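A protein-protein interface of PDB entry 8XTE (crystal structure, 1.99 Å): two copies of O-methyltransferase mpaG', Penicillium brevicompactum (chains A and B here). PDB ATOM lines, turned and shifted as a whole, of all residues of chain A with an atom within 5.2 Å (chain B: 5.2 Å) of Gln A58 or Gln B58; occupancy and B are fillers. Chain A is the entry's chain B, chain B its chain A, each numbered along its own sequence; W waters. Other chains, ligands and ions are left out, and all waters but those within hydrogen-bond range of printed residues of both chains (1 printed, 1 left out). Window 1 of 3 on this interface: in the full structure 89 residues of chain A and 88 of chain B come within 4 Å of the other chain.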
ATOM      1  N   GLN A  52     -24.922  -5.195  10.376  1.00  0.00           N
ATOM      2  CA  GLN A  52     -24.498  -4.924   9.005  1.00  0.00           C
ATOM      3  C   GLN A  52     -23.102  -4.312   8.956  1.00  0.00           C
ATOM      4  O   GLN A  52     -22.305  -4.646   8.073  1.00  0.00           O
ATOM      5  CB  GLN A  52     -25.508  -4.011   8.308  1.00  0.00           C
ATOM      6  CG  GLN A  52     -26.838  -4.686   7.987  1.00  0.00           C
ATOM      7  CD  GLN A  52     -27.629  -3.922   6.945  1.00  0.00           C
ATOM      8  OE1 GLN A  52     -27.095  -3.038   6.271  1.00  0.00           O
ATOM      9  NE2 GLN A  52     -28.907  -4.264   6.798  1.00  0.00           N
ATOM     10  N   HIS A  53     -22.778  -3.414   9.888  1.00  0.00           N
ATOM     11  CA  HIS A  53     -21.440  -2.827   9.857  1.00  0.00           C
ATOM     12  C   HIS A  53     -20.374  -3.836  10.272  1.00  0.00           C
ATOM     13  O   HIS A  53     -19.310  -3.911   9.649  1.00  0.00           O
ATOM     14  CB  HIS A  53     -21.374  -1.584  10.745  1.00  0.00           C
ATOM     15  CG  HIS A  53     -20.022  -0.937  10.772  1.00  0.00           C
ATOM     16  ND1 HIS A  53     -19.128  -1.126  11.805  1.00  0.00           N
ATOM     17  CD2 HIS A  53     -19.400  -0.128   9.882  1.00  0.00           C
ATOM     18  CE1 HIS A  53     -18.021  -0.448  11.557  1.00  0.00           C
ATOM     19  NE2 HIS A  53     -18.160   0.163  10.394  1.00  0.00           N
ATOM     20  N   THR A  54     -20.642  -4.626  11.316  1.00  0.00           N
ATOM     21  CA  THR A  54     -19.623  -5.529  11.846  1.00  0.00           C
ATOM     22  C   THR A  54     -19.379  -6.719  10.923  1.00  0.00           C
ATOM     23  O   THR A  54     -18.227  -7.104  10.693  1.00  0.00           O
ATOM     24  CB  THR A  54     -20.027  -6.006  13.244  1.00  0.00           C
ATOM     25  OG1 THR A  54     -20.185  -4.869  14.103  1.00  0.00           O
ATOM     26  CG2 THR A  54     -18.975  -6.947  13.825  1.00  0.00           C
ATOM     27  N   TRP A  56     -20.999  -7.290   7.637  1.00  0.00           N
ATOM     28  CA  TRP A  56     -21.065  -7.044   6.199  1.00  0.00           C
ATOM     29  C   TRP A  56     -20.026  -6.021   5.757  1.00  0.00           C
ATOM     30  O   TRP A  56     -19.157  -6.330   4.935  1.00  0.00           O
ATOM     31  CB  TRP A  56     -22.460  -6.559   5.764  1.00  0.00           C
ATOM     32  CG  TRP A  56     -23.654  -7.357   6.214  1.00  0.00           C
ATOM     33  CD1 TRP A  56     -23.680  -8.409   7.090  1.00  0.00           C
ATOM     34  CD2 TRP A  56     -25.014  -7.141   5.811  1.00  0.00           C
ATOM     35  NE1 TRP A  56     -24.971  -8.859   7.251  1.00  0.00           N
ATOM     36  CE2 TRP A  56     -25.806  -8.100   6.472  1.00  0.00           C
ATOM     37  CE3 TRP A  56     -25.636  -6.232   4.946  1.00  0.00           C
ATOM     38  CZ2 TRP A  56     -27.189  -8.174   6.295  1.00  0.00           C
ATOM     39  CZ3 TRP A  56     -27.003  -6.311   4.770  1.00  0.00           C
ATOM     40  CH2 TRP A  56     -27.766  -7.272   5.443  1.00  0.00           C
ATOM     41  N   SER A  57     -20.097  -4.798   6.288  1.00  0.00           N
ATOM     42  CA  SER A  57     -19.286  -3.704   5.763  1.00  0.00           C
ATOM     43  C   SER A  57     -17.801  -3.940   5.999  1.00  0.00           C
ATOM     44  O   SER A  57     -16.987  -3.792   5.081  1.00  0.00           O
ATOM     45  CB  SER A  57     -19.723  -2.383   6.393  1.00  0.00           C
ATOM     46  OG  SER A  57     -21.124  -2.233   6.278  1.00  0.00           O
ATOM     47  N   GLN A  58     -17.424  -4.297   7.230  1.00  0.00           N
ATOM     48  CA  GLN A  58     -16.000  -4.405   7.543  1.00  0.00           C
ATOM     49  C   GLN A  58     -15.348  -5.614   6.886  1.00  0.00           C
ATOM     50  O   GLN A  58     -14.244  -5.465   6.336  1.00  0.00           O
ATOM     51  CB  GLN A  58     -15.795  -4.399   9.063  1.00  0.00           C
ATOM     52  CG  GLN A  58     -15.961  -3.030   9.713  1.00  0.00           C
ATOM     53  CD  GLN A  58     -14.880  -2.032   9.314  1.00  0.00           C
ATOM     54  OE1 GLN A  58     -13.803  -2.408   8.859  1.00  0.00           O
ATOM     55  NE2 GLN A  58     -15.159  -0.754   9.520  1.00  0.00           N
ATOM     56  N   PRO A  59     -15.934  -6.820   6.907  1.00  0.00           N
ATOM     57  CA  PRO A  59     -15.287  -7.929   6.183  1.00  0.00           C
ATOM     58  C   PRO A  59     -15.160  -7.669   4.694  1.00  0.00           C
ATOM     59  O   PRO A  59     -14.165  -8.071   4.077  1.00  0.00           O
ATOM     60  CB  PRO A  59     -16.205  -9.123   6.483  1.00  0.00           C
ATOM     61  CG  PRO A  59     -16.835  -8.781   7.797  1.00  0.00           C
ATOM     62  CD  PRO A  59     -17.069  -7.299   7.722  1.00  0.00           C
ATOM     63  N   ALA A  60     -16.144  -6.993   4.099  1.00  0.00           N
ATOM     64  CA  ALA A  60     -16.051  -6.652   2.684  1.00  0.00           C
ATOM     65  C   ALA A  60     -14.976  -5.595   2.443  1.00  0.00           C
ATOM     66  O   ALA A  60     -14.247  -5.661   1.445  1.00  0.00           O
ATOM     67  CB  ALA A  60     -17.409  -6.179   2.174  1.00  0.00           C
ATOM     68  N   LEU A  61     -14.858  -4.620   3.348  1.00  0.00           N
ATOM     69  CA  LEU A  61     -13.774  -3.646   3.258  1.00  0.00           C
ATOM     70  C   LEU A  61     -12.417  -4.333   3.331  1.00  0.00           C
ATOM     71  O   LEU A  61     -11.523  -4.054   2.521  1.00  0.00           O
ATOM     72  CB  LEU A  61     -13.909  -2.601   4.370  1.00  0.00           C
ATOM     73  CG  LEU A  61     -12.822  -1.518   4.424  1.00  0.00           C
ATOM     74  CD1 LEU A  61     -12.792  -0.698   3.135  1.00  0.00           C
ATOM     75  CD2 LEU A  61     -13.006  -0.611   5.636  1.00  0.00           C
ATOM     76  N   SER A  62     -12.241  -5.232   4.307  1.00  0.00           N
ATOM     77  CA  SER A  62     -10.989  -5.980   4.421  1.00  0.00           C
ATOM     78  C   SER A  62     -10.669  -6.716   3.126  1.00  0.00           C
ATOM     79  O   SER A  62      -9.530  -6.682   2.644  1.00  0.00           O
ATOM     80  CB  SER A  62     -11.069  -6.971   5.584  1.00  0.00           C
ATOM     81  OG  SER A  62     -11.018  -6.303   6.826  1.00  0.00           O
ATOM     82  N   ALA A  63     -11.670  -7.388   2.550  1.00  0.00           N
ATOM     83  CA  ALA A  63     -11.457  -8.176   1.339  1.00  0.00           C
ATOM     84  C   ALA A  63     -11.079  -7.293   0.155  1.00  0.00           C
ATOM     85  O   ALA A  63     -10.156  -7.620  -0.601  1.00  0.00           O
ATOM     86  CB  ALA A  63     -12.711  -8.992   1.016  1.00  0.00           C
ATOM     87  N   HIS A 107     -18.105   0.500  -2.702  1.00  0.00           N
ATOM     88  CA  HIS A 107     -18.002   0.216  -1.273  1.00  0.00           C
ATOM     89  C   HIS A 107     -16.865   1.011  -0.643  1.00  0.00           C
ATOM     90  O   HIS A 107     -17.006   1.525   0.473  1.00  0.00           O
ATOM     91  CB  HIS A 107     -17.803  -1.280  -1.023  1.00  0.00           C
ATOM     92  CG  HIS A 107     -17.993  -1.677   0.412  1.00  0.00           C
ATOM     93  ND1 HIS A 107     -19.161  -1.437   1.105  1.00  0.00           N
ATOM     94  CD2 HIS A 107     -17.149  -2.266   1.294  1.00  0.00           C
ATOM     95  CE1 HIS A 107     -19.036  -1.877   2.345  1.00  0.00           C
ATOM     96  NE2 HIS A 107     -17.822  -2.383   2.487  1.00  0.00           N
ATOM     97  N   MET A 111     -17.241   3.523   2.402  1.00  0.00           N
ATOM     98  CA  MET A 111     -16.426   3.335   3.598  1.00  0.00           C
ATOM     99  C   MET A 111     -15.432   4.464   3.830  1.00  0.00           C
ATOM    100  O   MET A 111     -14.661   4.389   4.792  1.00  0.00           O
ATOM    101  CB  MET A 111     -15.671   2.003   3.516  1.00  0.00           C
ATOM    102  CG  MET A 111     -16.553   0.756   3.572  1.00  0.00           C
ATOM    103  SD  MET A 111     -17.616   0.676   5.035  1.00  0.00           S
ATOM    104  CE  MET A 111     -16.418   0.933   6.340  1.00  0.00           C
ATOM    105  N   GLN B  52      -5.070  -0.780  11.947  1.00  0.00           N
ATOM    106  CA  GLN B  52      -5.395  -1.454  13.204  1.00  0.00           C
ATOM    107  C   GLN B  52      -6.901  -1.608  13.397  1.00  0.00           C
ATOM    108  O   GLN B  52      -7.355  -2.606  13.964  1.00  0.00           O
ATOM    109  CB  GLN B  52      -4.787  -0.689  14.378  1.00  0.00           C
ATOM    110  CG  GLN B  52      -3.265  -0.721  14.435  1.00  0.00           C
ATOM    111  CD  GLN B  52      -2.750  -0.338  15.805  1.00  0.00           C
ATOM    112  OE1 GLN B  52      -3.535  -0.189  16.752  1.00  0.00           O
ATOM    113  NE2 GLN B  52      -1.433  -0.197  15.931  1.00  0.00           N
ATOM    114  N   HIS B  53      -7.698  -0.634  12.952  1.00  0.00           N
ATOM    115  CA  HIS B  53      -9.143  -0.750  13.133  1.00  0.00           C
ATOM    116  C   HIS B  53      -9.736  -1.762  12.160  1.00  0.00           C
ATOM    117  O   HIS B  53     -10.487  -2.660  12.562  1.00  0.00           O
ATOM    118  CB  HIS B  53      -9.815   0.613  12.968  1.00  0.00           C
ATOM    119  CG  HIS B  53     -11.297   0.585  13.185  1.00  0.00           C
ATOM    120  ND1 HIS B  53     -12.203   0.527  12.147  1.00  0.00           N
ATOM    121  CD2 HIS B  53     -12.031   0.602  14.324  1.00  0.00           C
ATOM    122  CE1 HIS B  53     -13.430   0.518  12.636  1.00  0.00           C
ATOM    123  NE2 HIS B  53     -13.354   0.564  13.955  1.00  0.00           N
ATOM    124  N   THR B  54      -9.389  -1.642  10.875  1.00  0.00           N
ATOM    125  CA  THR B  54      -9.942  -2.525   9.852  1.00  0.00           C
ATOM    126  C   THR B  54      -9.472  -3.966  10.028  1.00  0.00           C
ATOM    127  O   THR B  54     -10.258  -4.906   9.854  1.00  0.00           O
ATOM    128  CB  THR B  54      -9.559  -2.001   8.465  1.00  0.00           C
ATOM    129  OG1 THR B  54     -10.106  -0.688   8.286  1.00  0.00           O
ATOM    130  CG2 THR B  54     -10.065  -2.927   7.359  1.00  0.00           C
ATOM    131  N   TRP B  56      -7.479  -5.344  12.819  1.00  0.00           N
ATOM    132  CA  TRP B  56      -7.386  -5.886  14.173  1.00  0.00           C
ATOM    133  C   TRP B  56      -8.701  -5.730  14.930  1.00  0.00           C
ATOM    134  O   TRP B  56      -9.300  -6.730  15.332  1.00  0.00           O
ATOM    135  CB  TRP B  56      -6.253  -5.229  14.989  1.00  0.00           C
ATOM    136  CG  TRP B  56      -4.896  -5.059  14.334  1.00  0.00           C
ATOM    137  CD1 TRP B  56      -4.533  -5.390  13.058  1.00  0.00           C
ATOM    138  CD2 TRP B  56      -3.724  -4.493  14.947  1.00  0.00           C
ATOM    139  NE1 TRP B  56      -3.208  -5.073  12.843  1.00  0.00           N
ATOM    140  CE2 TRP B  56      -2.692  -4.519  13.986  1.00  0.00           C
ATOM    141  CE3 TRP B  56      -3.451  -3.973  16.216  1.00  0.00           C
ATOM    142  CZ2 TRP B  56      -1.404  -4.047  14.257  1.00  0.00           C
ATOM    143  CZ3 TRP B  56      -2.175  -3.506  16.485  1.00  0.00           C
ATOM    144  CH2 TRP B  56      -1.167  -3.543  15.507  1.00  0.00           C
ATOM    145  N   SER B  57      -9.170  -4.492  15.127  1.00  0.00           N
ATOM    146  CA  SER B  57     -10.330  -4.246  15.986  1.00  0.00           C
ATOM    147  C   SER B  57     -11.575  -4.972  15.486  1.00  0.00           C
ATOM    148  O   SER B  57     -12.306  -5.586  16.274  1.00  0.00           O
ATOM    149  CB  SER B  57     -10.603  -2.744  16.080  1.00  0.00           C
ATOM    150  OG  SER B  57      -9.399  -2.002  16.079  1.00  0.00           O
ATOM    151  N   GLN B  58     -11.843  -4.898  14.186  1.00  0.00           N
ATOM    152  CA  GLN B  58     -13.105  -5.400  13.653  1.00  0.00           C
ATOM    153  C   GLN B  58     -13.118  -6.926  13.537  1.00  0.00           C
ATOM    154  O   GLN B  58     -14.091  -7.555  13.972  1.00  0.00           O
ATOM    155  CB  GLN B  58     -13.412  -4.734  12.307  1.00  0.00           C
ATOM    156  CG  GLN B  58     -13.718  -3.244  12.432  1.00  0.00           C
ATOM    157  CD  GLN B  58     -15.006  -2.968  13.200  1.00  0.00           C
ATOM    158  OE1 GLN B  58     -15.962  -3.741  13.142  1.00  0.00           O
ATOM    159  NE2 GLN B  58     -15.025  -1.867  13.936  1.00  0.00           N
ATOM    160  N   PRO B  59     -12.090  -7.572  12.971  1.00  0.00           N
ATOM    161  CA  PRO B  59     -12.083  -9.048  13.001  1.00  0.00           C
ATOM    162  C   PRO B  59     -12.064  -9.616  14.410  1.00  0.00           C
ATOM    163  O   PRO B  59     -12.653 -10.680  14.653  1.00  0.00           O
ATOM    164  CB  PRO B  59     -10.805  -9.412  12.231  1.00  0.00           C
ATOM    165  CG  PRO B  59     -10.524  -8.225  11.386  1.00  0.00           C
ATOM    166  CD  PRO B  59     -10.937  -7.050  12.213  1.00  0.00           C
ATOM    167  N   ALA B  60     -11.394  -8.938  15.347  1.00  0.00           N
ATOM    168  CA  ALA B  60     -11.445  -9.367  16.739  1.00  0.00           C
ATOM    169  C   ALA B  60     -12.837  -9.158  17.319  1.00  0.00           C
ATOM    170  O   ALA B  60     -13.353 -10.027  18.031  1.00  0.00           O
ATOM    171  CB  ALA B  60     -10.400  -8.617  17.559  1.00  0.00           C
ATOM    172  N   LEU B  61     -13.462  -8.018  17.015  1.00  0.00           N
ATOM    173  CA  LEU B  61     -14.831  -7.764  17.459  1.00  0.00           C
ATOM    174  C   LEU B  61     -15.793  -8.828  16.940  1.00  0.00           C
ATOM    175  O   LEU B  61     -16.627  -9.343  17.694  1.00  0.00           O
ATOM    176  CB  LEU B  61     -15.278  -6.376  17.007  1.00  0.00           C
ATOM    177  CG  LEU B  61     -16.692  -5.973  17.415  1.00  0.00           C
ATOM    178  CD1 LEU B  61     -16.812  -5.938  18.938  1.00  0.00           C
ATOM    179  CD2 LEU B  61     -17.060  -4.630  16.799  1.00  0.00           C
ATOM    180  N   SER B  62     -15.700  -9.159  15.646  1.00  0.00           N
ATOM    181  CA  SER B  62     -16.589 -10.163  15.062  1.00  0.00           C
ATOM    182  C   SER B  62     -16.493 -11.485  15.813  1.00  0.00           C
ATOM    183  O   SER B  62     -17.513 -12.099  16.144  1.00  0.00           O
ATOM    184  CB  SER B  62     -16.252 -10.376  13.583  1.00  0.00           C
ATOM    185  OG  SER B  62     -16.487  -9.205  12.820  1.00  0.00           O
ATOM    186  N   ALA B  63     -15.268 -11.932  16.096  1.00  0.00           N
ATOM    187  CA  ALA B  63     -15.070 -13.236  16.724  1.00  0.00           C
ATOM    188  C   ALA B  63     -15.550 -13.244  18.169  1.00  0.00           C
ATOM    189  O   ALA B  63     -16.116 -14.243  18.629  1.00  0.00           O
ATOM    190  CB  ALA B  63     -13.597 -13.629  16.652  1.00  0.00           C
ATOM    191  N   HIS B 107     -12.222  -5.688  25.161  1.00  0.00           N
ATOM    192  CA  HIS B 107     -12.363  -5.264  23.771  1.00  0.00           C
ATOM    193  C   HIS B 107     -13.809  -4.899  23.435  1.00  0.00           C
ATOM    194  O   HIS B 107     -14.047  -3.973  22.650  1.00  0.00           O
ATOM    195  CB  HIS B 107     -11.849  -6.355  22.832  1.00  0.00           C
ATOM    196  CG  HIS B 107     -11.668  -5.897  21.417  1.00  0.00           C
ATOM    197  ND1 HIS B 107     -10.711  -4.976  21.049  1.00  0.00           N
ATOM    198  CD2 HIS B 107     -12.328  -6.229  20.280  1.00  0.00           C
ATOM    199  CE1 HIS B 107     -10.788  -4.761  19.747  1.00  0.00           C
ATOM    200  NE2 HIS B 107     -11.760  -5.511  19.257  1.00  0.00           N
ATOM    201  N   MET B 111     -14.779  -1.208  22.213  1.00  0.00           N
ATOM    202  CA  MET B 111     -15.515  -1.106  20.962  1.00  0.00           C
ATOM    203  C   MET B 111     -16.945  -0.625  21.170  1.00  0.00           C
ATOM    204  O   MET B 111     -17.709  -0.572  20.202  1.00  0.00           O
ATOM    205  CB  MET B 111     -15.526  -2.458  20.239  1.00  0.00           C
ATOM    206  CG  MET B 111     -14.149  -2.931  19.773  1.00  0.00           C
ATOM    207  SD  MET B 111     -13.309  -1.814  18.642  1.00  0.00           S
ATOM    208  CE  MET B 111     -14.070  -2.267  17.086  1.00  0.00           C
HETATM  209  O   HOH W   1     -18.978  -2.724  13.872  1.00  0.00           O
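Water W1 lies within hydrogen-bond range of OG1 of Thr A54 (2.5 Å), ND1 of His A53 (2.6 Å) and OE1 of Gln B58 (3.3 Å).
Thr A54 touches Ser B62, and with the chains exchanged Ser A62 touches Thr B54.
Gln A58 touches His B53, but with the chains exchanged His A53 does not touch Gln B58 (4.1 Å).
Gln A58 touches its own counterpart, Gln B58.
Leu A61 touches Thr B54, but with the chains exchanged Thr A54 does not touch Leu B61 (4.1 Å).
Positions printed for both chains: 52, 53, 54, 56, 57, 58, 59, 60, 61, 62, 63, 107 and 111.
Printed residues of chain A that touch a printed residue of chain B: Thr A54, Gln A58, Leu A61 and Ser A62.
Of the 13 printed residues of chain B, 4 touch a printed residue of chain A.
Hydrophobic or aromatic side chains of chain B that line the printed part of chain A: His B53.
NE2 of His B53 is in hydrogen-bond range of NE2 of Gln B58 (2.9 Å).
O of Gln B58 lies within hydrogen-bond range of OG of Ser B62 (3.1 Å).
The backbone carbonyl oxygen of His A53 is in hydrogen-bond range of the backbone NH of Gln A58, 3.1 Å away.
The backbone carbonyl oxygen (O) of Gln A58 lies within hydrogen-bond range of the side-chain hydroxyl (OG) of Ser A62, 3.4 Å away.
Of the printed residues of chain B, Gln A58 touches His B53 (3.8 Å), Thr B54 (3.99 Å) and Gln B58 (3.5 Å).
Of chain A, only Gln A58 (3.5 Å) comes within 4 Å of Gln B58.
Printed residues of chain A within 4 Å of Thr B54: Gln A58, Leu A61 and Ser A62.
Printed residues of chain B within 4 Å of Thr A54: Ser B62.
Of the printed residues of chain B, Ser A62 touches Thr B54 (3.4 Å).
Printed residues of chain A within 4 Å of Ser B62: Thr A54.
Met B111 touches none of the printed residues of chain A.
His B107 touches none of the printed residues of chain A.
The backbone carbonyl oxygen (O) of Thr B54 is in hydrogen-bond range of the side-chain hydroxyl (OG) of Ser A62 (3.4 Å).
The side-chain hydroxyl (OG) of Ser B62 lies within hydrogen-bond range of the backbone carbonyl oxygen (O) of Thr A54 (3.5 Å).
Among the printed residues, merely in contact across the chains: Gln A58 with His B53, Gln A58 with Thr B54, Gln A58 with Gln B58 and Leu A61 with Thr B54.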
